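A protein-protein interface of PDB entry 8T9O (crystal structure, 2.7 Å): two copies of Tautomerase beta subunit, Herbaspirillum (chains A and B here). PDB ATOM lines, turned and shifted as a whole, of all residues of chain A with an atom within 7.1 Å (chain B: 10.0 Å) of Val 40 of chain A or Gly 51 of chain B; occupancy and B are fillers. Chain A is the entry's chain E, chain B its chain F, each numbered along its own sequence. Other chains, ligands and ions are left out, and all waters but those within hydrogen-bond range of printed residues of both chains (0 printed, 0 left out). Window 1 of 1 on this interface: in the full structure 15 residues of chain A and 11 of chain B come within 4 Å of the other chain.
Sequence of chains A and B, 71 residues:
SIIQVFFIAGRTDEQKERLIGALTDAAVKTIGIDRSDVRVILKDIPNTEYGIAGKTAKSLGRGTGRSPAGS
Of the 20 printed residues of chain B, 9 touch a printed residue of chain A.
Hydrophobic or aromatic side chains of chain B that line the printed part of chain A: Phe 6, Ile 45, Tyr 50, Ile 52 and Ala 53.
No residue of chain B comes within 4 Å of Ile 3 of chain A.
Val 5 of chain A touches none of the printed residues of chain B.
Of the printed residues of chain B, Arg 35 of chain A touches Ala 53.
Of the printed residues of chain B, Val 40 of chain A touches Glu 49 (3.7 Å), Tyr 50 (3.5 Å) and Gly 51 (2.9 Å).
Of the printed residues of chain B, Ile 41 of chain A touches Phe 6, Ile 45, Glu 49 and Tyr 50.
Of the printed residues of chain A, Phe 6 of chain B touches Gln 4 (3.1 Å) and Ile 41 (3.4 Å).
Gly 51 of chain B touches just these residues of chain A: Ile 20 (3.7 Å), Val 38 (3.6 Å), Arg 39 (3.1 Å) and Val 40 (2.9 Å).
The nearest residue of chain B that does not touch Val 40 of chain A is Ile 52 of chain B (5.2 Å).
The nearest residue of chain A that does not touch Gly 51 of chain B is Ile 41 of chain A (5.1 Å).
No position is printed for both chains.
Of the 22 pairs that touch across the chains among the printed residues, none has its exchanged pair printed and touching as well.
Lys 16 of chain A touches Thr 48 of chain B.
Gly 51 of chain B touches Ile 20 of chain A (CA to CG2, 3.7 Å).
Ile 20 of chain A touches Gly 54 of chain B.
O of Gly 54 of chain B touches CA of Gly 21 of chain A (3.5 Å).
Arg 39 of chain A touches Ile 52 of chain B.
Arg 39 of chain A touches Ala 53 of chain B.
Val 40 of chain A touches Glu 49 of chain B (O to O, 3.7 Å).
O of Val 40 of chain A touches CA of Tyr 50 of chain B (3.5 Å).
CG2 of Ile 41 of chain A touches CD2 of Phe 6 of chain B, at 3.4 Å.
C of Ile 41 of chain A touches O of Glu 49 of chain B, 3.9 Å away.
NZ of Lys 16 of chain A lies within salt-bridge range of OE2 of Glu 49 of chain B.
O of Ala 53 of chain B sits at hydrogen-bond distance from NH2 of Arg 35 of chain A, 3.5 Å away.
The backbone NH of Ala 53 of chain B lies within hydrogen-bond range of the backbone carbonyl oxygen of Val 38 of chain A, 3.4 Å away.
N of Gly 51 of chain B lies within hydrogen-bond range of O of Val 40 of chain A, 2.9 Å away.
The backbone carbonyl oxygen (O) of Glu 49 of chain B lies within hydrogen-bond range of the backbone NH (N) of Leu 42 of chain A (2.9 Å).
O of Ser 1 of chain A is in hydrogen-bond range of N of Arg 39 of chain A, at 3.1 Å.
The backbone carbonyl oxygen (O) of Arg 39 of chain A lies within hydrogen-bond range of the backbone NH (N) of Ile 3 of chain A, 2.8 Å away.
The backbone carbonyl oxygen (O) of Ile 3 of chain A is in hydrogen-bond range of the backbone NH (N) of Ile 41 of chain A (2.7 Å).
The backbone carbonyl oxygen (O) of Gly 21 of chain A lies within hydrogen-bond range of the side-chain hydroxyl (OG1) of Thr 24 of chain A, at 2.6 Å.
N of Ile 45 of chain B lies within hydrogen-bond range of O of Phe 7 of chain B (3.0 Å).
O of Tyr 50 of chain B lies within hydrogen-bond range of N of Ala 57 of chain B (2.9 Å).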
ATOM      1  N   SER A   1     -31.547 -11.386  20.871  1.00  0.00           N
ATOM      2  CA  SER A   1     -32.187 -10.503  19.906  1.00  0.00           C
ATOM      3  C   SER A   1     -31.419  -9.193  19.725  1.00  0.00           C
ATOM      4  O   SER A   1     -31.470  -8.589  18.659  1.00  0.00           O
ATOM      5  CB  SER A   1     -33.632 -10.215  20.326  1.00  0.00           C
ATOM      6  OG  SER A   1     -33.688  -9.631  21.614  1.00  0.00           O
ATOM      7  N   ILE A   2     -30.703  -8.750  20.755  1.00  0.00           N
ATOM      8  CA  ILE A   2     -29.964  -7.492  20.695  1.00  0.00           C
ATOM      9  C   ILE A   2     -28.489  -7.802  20.465  1.00  0.00           C
ATOM     10  O   ILE A   2     -27.875  -8.555  21.230  1.00  0.00           O
ATOM     11  CB  ILE A   2     -30.157  -6.645  21.966  1.00  0.00           C
ATOM     12  CG1 ILE A   2     -31.640  -6.449  22.286  1.00  0.00           C
ATOM     13  CG2 ILE A   2     -29.481  -5.293  21.810  1.00  0.00           C
ATOM     14  CD1 ILE A   2     -32.176  -7.440  23.278  1.00  0.00           C
ATOM     15  N   ILE A   3     -27.927  -7.213  19.411  1.00  0.00           N
ATOM     16  CA  ILE A   3     -26.522  -7.369  19.051  1.00  0.00           C
ATOM     17  C   ILE A   3     -25.821  -6.046  19.324  1.00  0.00           C
ATOM     18  O   ILE A   3     -26.315  -4.985  18.926  1.00  0.00           O
ATOM     19  CB  ILE A   3     -26.363  -7.777  17.576  1.00  0.00           C
ATOM     20  CG1 ILE A   3     -27.240  -8.990  17.251  1.00  0.00           C
ATOM     21  CG2 ILE A   3     -24.908  -8.087  17.260  1.00  0.00           C
ATOM     22  CD1 ILE A   3     -27.429  -9.224  15.763  1.00  0.00           C
ATOM     23  N   GLN A   4     -24.675  -6.106  19.998  1.00  0.00           N
ATOM     24  CA  GLN A   4     -23.904  -4.916  20.335  1.00  0.00           C
ATOM     25  C   GLN A   4     -22.480  -5.091  19.834  1.00  0.00           C
ATOM     26  O   GLN A   4     -21.833  -6.098  20.141  1.00  0.00           O
ATOM     27  CB  GLN A   4     -23.926  -4.664  21.847  1.00  0.00           C
ATOM     28  CG  GLN A   4     -23.321  -3.343  22.297  1.00  0.00           C
ATOM     29  CD  GLN A   4     -23.211  -3.261  23.807  1.00  0.00           C
ATOM     30  OE1 GLN A   4     -22.961  -2.197  24.370  1.00  0.00           O
ATOM     31  NE2 GLN A   4     -23.392  -4.392  24.473  1.00  0.00           N
ATOM     32  N   VAL A   5     -21.996  -4.116  19.068  1.00  0.00           N
ATOM     33  CA  VAL A   5     -20.674  -4.161  18.453  1.00  0.00           C
ATOM     34  C   VAL A   5     -19.814  -3.061  19.063  1.00  0.00           C
ATOM     35  O   VAL A   5     -20.233  -1.899  19.127  1.00  0.00           O
ATOM     36  CB  VAL A   5     -20.759  -4.008  16.924  1.00  0.00           C
ATOM     37  CG1 VAL A   5     -19.369  -3.891  16.316  1.00  0.00           C
ATOM     38  CG2 VAL A   5     -21.519  -5.176  16.308  1.00  0.00           C
ATOM     39  N   LYS A  16     -21.760   1.082   8.267  1.00  0.00           N
ATOM     40  CA  LYS A  16     -22.557   0.720   9.434  1.00  0.00           C
ATOM     41  C   LYS A  16     -23.960   0.289   9.028  1.00  0.00           C
ATOM     42  O   LYS A  16     -24.611  -0.475   9.750  1.00  0.00           O
ATOM     43  CB  LYS A  16     -22.623   1.900  10.402  1.00  0.00           C
ATOM     44  CG  LYS A  16     -21.259   2.381  10.870  1.00  0.00           C
ATOM     45  CD  LYS A  16     -21.370   3.699  11.613  1.00  0.00           C
ATOM     46  CE  LYS A  16     -20.007   4.340  11.803  1.00  0.00           C
ATOM     47  NZ  LYS A  16     -20.097   5.825  11.848  1.00  0.00           N
ATOM     48  N   LEU A  19     -23.451  -3.270   8.009  1.00  0.00           N
ATOM     49  CA  LEU A  19     -23.214  -4.037   9.227  1.00  0.00           C
ATOM     50  C   LEU A  19     -24.526  -4.374   9.922  1.00  0.00           C
ATOM     51  O   LEU A  19     -24.796  -5.542  10.227  1.00  0.00           O
ATOM     52  CB  LEU A  19     -22.285  -3.268  10.168  1.00  0.00           C
ATOM     53  CG  LEU A  19     -21.533  -4.119  11.195  1.00  0.00           C
ATOM     54  CD1 LEU A  19     -20.688  -5.170  10.506  1.00  0.00           C
ATOM     55  CD2 LEU A  19     -20.665  -3.252  12.098  1.00  0.00           C
ATOM     56  N   ILE A  20     -25.367  -3.362  10.157  1.00  0.00           N
ATOM     57  CA  ILE A  20     -26.652  -3.587  10.818  1.00  0.00           C
ATOM     58  C   ILE A  20     -27.466  -4.624  10.055  1.00  0.00           C
ATOM     59  O   ILE A  20     -28.019  -5.563  10.641  1.00  0.00           O
ATOM     60  CB  ILE A  20     -27.421  -2.261  10.960  1.00  0.00           C
ATOM     61  CG1 ILE A  20     -26.736  -1.348  11.979  1.00  0.00           C
ATOM     62  CG2 ILE A  20     -28.862  -2.526  11.358  1.00  0.00           C
ATOM     63  CD1 ILE A  20     -27.369   0.025  12.088  1.00  0.00           C
ATOM     64  N   GLY A  21     -27.538  -4.472   8.733  1.00  0.00           N
ATOM     65  CA  GLY A  21     -28.273  -5.437   7.931  1.00  0.00           C
ATOM     66  C   GLY A  21     -27.662  -6.824   7.983  1.00  0.00           C
ATOM     67  O   GLY A  21     -28.345  -7.803   8.301  1.00  0.00           O
ATOM     68  N   LEU A  23     -25.654  -8.269  10.058  1.00  0.00           N
ATOM     69  CA  LEU A  23     -25.728  -8.925  11.360  1.00  0.00           C
ATOM     70  C   LEU A  23     -27.129  -9.466  11.621  1.00  0.00           C
ATOM     71  O   LEU A  23     -27.298 -10.641  11.974  1.00  0.00           O
ATOM     72  CB  LEU A  23     -25.302  -7.953  12.458  1.00  0.00           C
ATOM     73  CG  LEU A  23     -23.814  -7.588  12.465  1.00  0.00           C
ATOM     74  CD1 LEU A  23     -23.493  -6.611  13.583  1.00  0.00           C
ATOM     75  CD2 LEU A  23     -22.964  -8.844  12.587  1.00  0.00           C
ATOM     76  N   THR A  24     -28.148  -8.617  11.451  1.00  0.00           N
ATOM     77  CA  THR A  24     -29.532  -9.075  11.555  1.00  0.00           C
ATOM     78  C   THR A  24     -29.824 -10.206  10.575  1.00  0.00           C
ATOM     79  O   THR A  24     -30.435 -11.215  10.944  1.00  0.00           O
ATOM     80  CB  THR A  24     -30.496  -7.910  11.325  1.00  0.00           C
ATOM     81  OG1 THR A  24     -30.206  -7.289  10.064  1.00  0.00           O
ATOM     82  CG2 THR A  24     -30.433  -6.895  12.445  1.00  0.00           C
ATOM     83  N   ARG A  35     -37.064 -10.872  12.167  1.00  0.00           N
ATOM     84  CA  ARG A  35     -36.282  -9.657  11.946  1.00  0.00           C
ATOM     85  C   ARG A  35     -36.693  -8.561  12.915  1.00  0.00           C
ATOM     86  O   ARG A  35     -35.845  -7.860  13.483  1.00  0.00           O
ATOM     87  CB  ARG A  35     -36.436  -9.135  10.516  1.00  0.00           C
ATOM     88  CG  ARG A  35     -35.935 -10.034   9.425  1.00  0.00           C
ATOM     89  CD  ARG A  35     -36.063  -9.318   8.088  1.00  0.00           C
ATOM     90  NE  ARG A  35     -35.060  -8.269   7.915  1.00  0.00           N
ATOM     91  CZ  ARG A  35     -33.816  -8.501   7.510  1.00  0.00           C
ATOM     92  NH1 ARG A  35     -33.421  -9.744   7.260  1.00  0.00           N
ATOM     93  NH2 ARG A  35     -32.960  -7.498   7.368  1.00  0.00           N
ATOM     94  N   VAL A  38     -35.028  -7.933  16.361  1.00  0.00           N
ATOM     95  CA  VAL A  38     -33.579  -7.787  16.444  1.00  0.00           C
ATOM     96  C   VAL A  38     -33.219  -6.308  16.446  1.00  0.00           C
ATOM     97  O   VAL A  38     -33.618  -5.560  15.544  1.00  0.00           O
ATOM     98  CB  VAL A  38     -32.867  -8.522  15.296  1.00  0.00           C
ATOM     99  CG1 VAL A  38     -31.357  -8.452  15.497  1.00  0.00           C
ATOM    100  CG2 VAL A  38     -33.340  -9.964  15.206  1.00  0.00           C
ATOM    101  N   ARG A  39     -32.457  -5.892  17.453  1.00  0.00           N
ATOM    102  CA  ARG A  39     -31.882  -4.558  17.521  1.00  0.00           C
ATOM    103  C   ARG A  39     -30.364  -4.670  17.461  1.00  0.00           C
ATOM    104  O   ARG A  39     -29.778  -5.564  18.077  1.00  0.00           O
ATOM    105  CB  ARG A  39     -32.303  -3.827  18.801  1.00  0.00           C
ATOM    106  CG  ARG A  39     -33.752  -4.048  19.204  1.00  0.00           C
ATOM    107  CD  ARG A  39     -34.687  -3.061  18.527  1.00  0.00           C
ATOM    108  NE  ARG A  39     -36.077  -3.502  18.600  1.00  0.00           N
ATOM    109  CZ  ARG A  39     -36.778  -3.936  17.558  1.00  0.00           C
ATOM    110  NH1 ARG A  39     -38.038  -4.321  17.716  1.00  0.00           N
ATOM    111  NH2 ARG A  39     -36.220  -3.984  16.356  1.00  0.00           N
ATOM    112  N   VAL A  40     -29.730  -3.766  16.719  1.00  0.00           N
ATOM    113  CA  VAL A  40     -28.275  -3.719  16.606  1.00  0.00           C
ATOM    114  C   VAL A  40     -27.797  -2.391  17.178  1.00  0.00           C
ATOM    115  O   VAL A  40     -28.129  -1.326  16.647  1.00  0.00           O
ATOM    116  CB  VAL A  40     -27.806  -3.897  15.154  1.00  0.00           C
ATOM    117  CG1 VAL A  40     -26.291  -3.915  15.073  1.00  0.00           C
ATOM    118  CG2 VAL A  40     -28.366  -5.176  14.582  1.00  0.00           C
ATOM    119  N   ILE A  41     -27.020  -2.453  18.256  1.00  0.00           N
ATOM    120  CA  ILE A  41     -26.438  -1.271  18.883  1.00  0.00           C
ATOM    121  C   ILE A  41     -24.997  -1.173  18.393  1.00  0.00           C
ATOM    122  O   ILE A  41     -24.195  -2.085  18.631  1.00  0.00           O
ATOM    123  CB  ILE A  41     -26.476  -1.373  20.416  1.00  0.00           C
ATOM    124  CG1 ILE A  41     -27.875  -1.740  20.929  1.00  0.00           C
ATOM    125  CG2 ILE A  41     -26.076  -0.032  21.024  1.00  0.00           C
ATOM    126  CD1 ILE A  41     -28.956  -0.742  20.640  1.00  0.00           C
ATOM    127  N   LEU A  42     -24.656  -0.084  17.708  1.00  0.00           N
ATOM    128  CA  LEU A  42     -23.306   0.124  17.191  1.00  0.00           C
ATOM    129  C   LEU A  42     -22.618   1.193  18.024  1.00  0.00           C
ATOM    130  O   LEU A  42     -23.108   2.320  18.121  1.00  0.00           O
ATOM    131  CB  LEU A  42     -23.318   0.536  15.720  1.00  0.00           C
ATOM    132  CG  LEU A  42     -23.712  -0.501  14.670  1.00  0.00           C
ATOM    133  CD1 LEU A  42     -23.312  -0.005  13.293  1.00  0.00           C
ATOM    134  CD2 LEU A  42     -23.076  -1.849  14.963  1.00  0.00           C
ATOM    135  N   PHE B   6     -29.801   1.860  26.380  1.00  0.00           N
ATOM    136  CA  PHE B   6     -29.380   2.148  25.017  1.00  0.00           C
ATOM    137  C   PHE B   6     -30.555   2.823  24.324  1.00  0.00           C
ATOM    138  O   PHE B   6     -31.632   2.227  24.224  1.00  0.00           O
ATOM    139  CB  PHE B   6     -29.006   0.863  24.279  1.00  0.00           C
ATOM    140  CG  PHE B   6     -27.891   0.083  24.918  1.00  0.00           C
ATOM    141  CD1 PHE B   6     -28.143  -0.723  26.017  1.00  0.00           C
ATOM    142  CD2 PHE B   6     -26.614   0.106  24.394  1.00  0.00           C
ATOM    143  CE1 PHE B   6     -27.134  -1.457  26.604  1.00  0.00           C
ATOM    144  CE2 PHE B   6     -25.597  -0.627  24.974  1.00  0.00           C
ATOM    145  CZ  PHE B   6     -25.858  -1.412  26.081  1.00  0.00           C
ATOM    146  N   PHE B   7     -30.372   4.058  23.861  1.00  0.00           N
ATOM    147  CA  PHE B   7     -31.524   4.745  23.298  1.00  0.00           C
ATOM    148  C   PHE B   7     -31.104   5.704  22.195  1.00  0.00           C
ATOM    149  O   PHE B   7     -29.988   6.233  22.192  1.00  0.00           O
ATOM    150  CB  PHE B   7     -32.337   5.443  24.403  1.00  0.00           C
ATOM    151  CG  PHE B   7     -31.655   6.617  25.062  1.00  0.00           C
ATOM    152  CD1 PHE B   7     -30.547   6.434  25.877  1.00  0.00           C
ATOM    153  CD2 PHE B   7     -32.203   7.888  24.972  1.00  0.00           C
ATOM    154  CE1 PHE B   7     -29.950   7.510  26.516  1.00  0.00           C
ATOM    155  CE2 PHE B   7     -31.617   8.963  25.616  1.00  0.00           C
ATOM    156  CZ  PHE B   7     -30.495   8.770  26.395  1.00  0.00           C
ATOM    157  N   ILE B   8     -32.021   5.890  21.239  1.00  0.00           N
ATOM    158  CA  ILE B   8     -31.742   6.689  20.056  1.00  0.00           C
ATOM    159  C   ILE B   8     -31.474   8.129  20.473  1.00  0.00           C
ATOM    160  O   ILE B   8     -32.063   8.648  21.432  1.00  0.00           O
ATOM    161  CB  ILE B   8     -32.902   6.612  19.043  1.00  0.00           C
ATOM    162  CG1 ILE B   8     -33.311   5.170  18.750  1.00  0.00           C
ATOM    163  CG2 ILE B   8     -32.523   7.240  17.735  1.00  0.00           C
ATOM    164  CD1 ILE B   8     -34.476   4.717  19.555  1.00  0.00           C
ATOM    165  N   ILE B  45     -27.309   6.696  20.944  1.00  0.00           N
ATOM    166  CA  ILE B  45     -26.775   6.081  19.739  1.00  0.00           C
ATOM    167  C   ILE B  45     -27.262   6.888  18.543  1.00  0.00           C
ATOM    168  O   ILE B  45     -28.470   7.091  18.386  1.00  0.00           O
ATOM    169  CB  ILE B  45     -27.175   4.602  19.604  1.00  0.00           C
ATOM    170  CG1 ILE B  45     -26.512   3.758  20.700  1.00  0.00           C
ATOM    171  CG2 ILE B  45     -26.812   4.088  18.234  1.00  0.00           C
ATOM    172  CD1 ILE B  45     -27.308   3.634  21.973  1.00  0.00           C
ATOM    173  N   PRO B  46     -26.363   7.386  17.692  1.00  0.00           N
ATOM    174  CA  PRO B  46     -26.798   8.124  16.501  1.00  0.00           C
ATOM    175  C   PRO B  46     -27.761   7.285  15.670  1.00  0.00           C
ATOM    176  O   PRO B  46     -27.727   6.054  15.706  1.00  0.00           O
ATOM    177  CB  PRO B  46     -25.496   8.395  15.733  1.00  0.00           C
ATOM    178  CG  PRO B  46     -24.380   8.085  16.670  1.00  0.00           C
ATOM    179  CD  PRO B  46     -24.903   7.302  17.824  1.00  0.00           C
ATOM    180  N   ASN B  47     -28.644   7.965  14.921  1.00  0.00           N
ATOM    181  CA  ASN B  47     -29.601   7.242  14.082  1.00  0.00           C
ATOM    182  C   ASN B  47     -28.910   6.295  13.115  1.00  0.00           C
ATOM    183  O   ASN B  47     -29.484   5.261  12.759  1.00  0.00           O
ATOM    184  CB  ASN B  47     -30.491   8.190  13.267  1.00  0.00           C
ATOM    185  CG  ASN B  47     -31.471   8.976  14.120  1.00  0.00           C
ATOM    186  OD1 ASN B  47     -32.298   9.723  13.598  1.00  0.00           O
ATOM    187  ND2 ASN B  47     -31.342   8.863  15.432  1.00  0.00           N
ATOM    188  N   THR B  48     -27.696   6.622  12.681  1.00  0.00           N
ATOM    189  CA  THR B  48     -26.956   5.819  11.721  1.00  0.00           C
ATOM    190  C   THR B  48     -26.221   4.650  12.367  1.00  0.00           C
ATOM    191  O   THR B  48     -25.445   3.971  11.688  1.00  0.00           O
ATOM    192  CB  THR B  48     -25.964   6.707  10.971  1.00  0.00           C
ATOM    193  OG1 THR B  48     -25.151   7.417  11.914  1.00  0.00           O
ATOM    194  CG2 THR B  48     -26.712   7.709  10.107  1.00  0.00           C
ATOM    195  N   GLU B  49     -26.446   4.403  13.660  1.00  0.00           N
ATOM    196  CA  GLU B  49     -25.747   3.348  14.383  1.00  0.00           C
ATOM    197  C   GLU B  49     -26.709   2.546  15.257  1.00  0.00           C
ATOM    198  O   GLU B  49     -26.265   1.795  16.134  1.00  0.00           O
ATOM    199  CB  GLU B  49     -24.599   3.967  15.194  1.00  0.00           C
ATOM    200  CG  GLU B  49     -23.604   4.674  14.253  1.00  0.00           C
ATOM    201  CD  GLU B  49     -22.457   5.409  14.922  1.00  0.00           C
ATOM    202  OE1 GLU B  49     -22.420   5.493  16.171  1.00  0.00           O
ATOM    203  OE2 GLU B  49     -21.596   5.931  14.181  1.00  0.00           O
ATOM    204  N   TYR B  50     -28.013   2.669  15.007  1.00  0.00           N
ATOM    205  CA  TYR B  50     -29.072   1.963  15.720  1.00  0.00           C
ATOM    206  C   TYR B  50     -29.900   1.184  14.707  1.00  0.00           C
ATOM    207  O   TYR B  50     -30.304   1.738  13.679  1.00  0.00           O
ATOM    208  CB  TYR B  50     -29.954   2.954  16.482  1.00  0.00           C
ATOM    209  CG  TYR B  50     -30.827   2.346  17.554  1.00  0.00           C
ATOM    210  CD1 TYR B  50     -31.967   1.624  17.224  1.00  0.00           C
ATOM    211  CD2 TYR B  50     -30.526   2.515  18.897  1.00  0.00           C
ATOM    212  CE1 TYR B  50     -32.772   1.074  18.202  1.00  0.00           C
ATOM    213  CE2 TYR B  50     -31.325   1.971  19.883  1.00  0.00           C
ATOM    214  CZ  TYR B  50     -32.446   1.251  19.529  1.00  0.00           C
ATOM    215  OH  TYR B  50     -33.245   0.706  20.507  1.00  0.00           O
ATOM    216  N   GLY B  51     -30.166  -0.087  14.998  1.00  0.00           N
ATOM    217  CA  GLY B  51     -30.816  -0.935  14.019  1.00  0.00           C
ATOM    218  C   GLY B  51     -32.139  -1.550  14.433  1.00  0.00           C
ATOM    219  O   GLY B  51     -32.235  -2.186  15.486  1.00  0.00           O
ATOM    220  N   ILE B  52     -33.166  -1.365  13.605  1.00  0.00           N
ATOM    221  CA  ILE B  52     -34.455  -2.033  13.761  1.00  0.00           C
ATOM    222  C   ILE B  52     -34.679  -2.878  12.519  1.00  0.00           C
ATOM    223  O   ILE B  52     -34.733  -2.342  11.405  1.00  0.00           O
ATOM    224  CB  ILE B  52     -35.616  -1.041  13.947  1.00  0.00           C
ATOM    225  CG1 ILE B  52     -35.402  -0.145  15.169  1.00  0.00           C
ATOM    226  CG2 ILE B  52     -36.949  -1.779  14.035  1.00  0.00           C
ATOM    227  CD1 ILE B  52     -34.739   1.172  14.840  1.00  0.00           C
ATOM    228  N   ALA B  53     -34.812  -4.191  12.711  1.00  0.00           N
ATOM    229  CA  ALA B  53     -35.027  -5.132  11.609  1.00  0.00           C
ATOM    230  C   ALA B  53     -33.986  -4.941  10.509  1.00  0.00           C
ATOM    231  O   ALA B  53     -34.296  -4.974   9.318  1.00  0.00           O
ATOM    232  CB  ALA B  53     -36.444  -5.008  11.048  1.00  0.00           C
ATOM    233  N   GLY B  54     -32.738  -4.719  10.917  1.00  0.00           N
ATOM    234  CA  GLY B  54     -31.660  -4.579   9.955  1.00  0.00           C
ATOM    235  C   GLY B  54     -31.651  -3.279   9.191  1.00  0.00           C
ATOM    236  O   GLY B  54     -30.906  -3.149   8.218  1.00  0.00           O
ATOM    237  N   LYS B  55     -32.463  -2.312   9.599  1.00  0.00           N
ATOM    238  CA  LYS B  55     -32.493  -0.997   8.982  1.00  0.00           C
ATOM    239  C   LYS B  55     -32.029   0.042   9.990  1.00  0.00           C
ATOM    240  O   LYS B  55     -32.181  -0.135  11.201  1.00  0.00           O
ATOM    241  CB  LYS B  55     -33.898  -0.659   8.495  1.00  0.00           C
ATOM    242  CG  LYS B  55     -34.416  -1.638   7.483  1.00  0.00           C
ATOM    243  CD  LYS B  55     -35.854  -1.355   7.214  1.00  0.00           C
ATOM    244  CE  LYS B  55     -36.457  -2.414   6.349  1.00  0.00           C
ATOM    245  NZ  LYS B  55     -37.848  -2.020   6.135  1.00  0.00           N
ATOM    246  N   THR B  56     -31.459   1.128   9.485  1.00  0.00           N
ATOM    247  CA  THR B  56     -30.960   2.156  10.383  1.00  0.00           C
ATOM    248  C   THR B  56     -32.100   3.050  10.855  1.00  0.00           C
ATOM    249  O   THR B  56     -33.100   3.246  10.159  1.00  0.00           O
ATOM    250  CB  THR B  56     -29.869   2.993   9.711  1.00  0.00           C
ATOM    251  OG1 THR B  56     -29.376   3.963  10.643  1.00  0.00           O
ATOM    252  CG2 THR B  56     -30.403   3.705   8.468  1.00  0.00           C
ATOM    253  N   ALA B  57     -31.938   3.582  12.067  1.00  0.00           N
ATOM    254  CA  ALA B  57     -32.940   4.469  12.646  1.00  0.00           C
ATOM    255  C   ALA B  57     -33.123   5.741  11.830  1.00  0.00           C
ATOM    256  O   ALA B  57     -34.152   6.412  11.966  1.00  0.00           O
ATOM    257  CB  ALA B  57     -32.555   4.816  14.085  1.00  0.00           C
ATOM    258  N   LYS B  58     -32.147   6.091  10.994  1.00  0.00           N
ATOM    259  CA  LYS B  58     -32.310   7.227  10.097  1.00  0.00           C
ATOM    260  C   LYS B  58     -33.360   6.927   9.036  1.00  0.00           C
ATOM    261  O   LYS B  58     -34.365   7.638   8.915  1.00  0.00           O
ATOM    262  CB  LYS B  58     -30.970   7.574   9.447  1.00  0.00           C
ATOM    263  CG  LYS B  58     -30.971   8.890   8.697  1.00  0.00           C
ATOM    264  CD  LYS B  58     -29.563   9.442   8.549  1.00  0.00           C
ATOM    265  CE  LYS B  58     -29.391  10.186   7.235  1.00  0.00           C
ATOM    266  NZ  LYS B  58     -28.190  11.066   7.251  1.00  0.00           N
ATOM    267  N   SER B  59     -33.151   5.852   8.273  1.00  0.00           N
ATOM    268  CA  SER B  59     -34.026   5.525   7.154  1.00  0.00           C
ATOM    269  C   SER B  59     -35.410   5.070   7.598  1.00  0.00           C
ATOM    270  O   SER B  59     -36.344   5.113   6.790  1.00  0.00           O
ATOM    271  CB  SER B  59     -33.384   4.445   6.282  1.00  0.00           C
ATOM    272  OG  SER B  59     -33.242   3.224   6.988  1.00  0.00           O
ATOM    273  N   LEU B  60     -35.569   4.627   8.849  1.00  0.00           N
ATOM    274  CA  LEU B  60     -36.895   4.246   9.356  1.00  0.00           C
ATOM    275  C   LEU B  60     -37.536   5.441  10.054  1.00  0.00           C
ATOM    276  O   LEU B  60     -38.548   5.973   9.589  1.00  0.00           O
ATOM    277  CB  LEU B  60     -36.785   3.036  10.288  1.00  0.00           C
ATOM    278  CG  LEU B  60     -38.077   2.283  10.677  1.00  0.00           C
ATOM    279  CD1 LEU B  60     -37.774   0.825  10.987  1.00  0.00           C
ATOM    280  CD2 LEU B  60     -38.817   2.926  11.851  1.00  0.00           C
ATOM    281  N   GLY B  61     -36.955   5.869  11.170  1.00  0.00           N
ATOM    282  CA  GLY B  61     -37.471   7.003  11.915  1.00  0.00           C
ATOM    283  C   GLY B  61     -36.814   7.167  13.270  1.00  0.00           C
ATOM    284  O   GLY B  61     -36.569   6.181  13.967  1.00  0.00           O
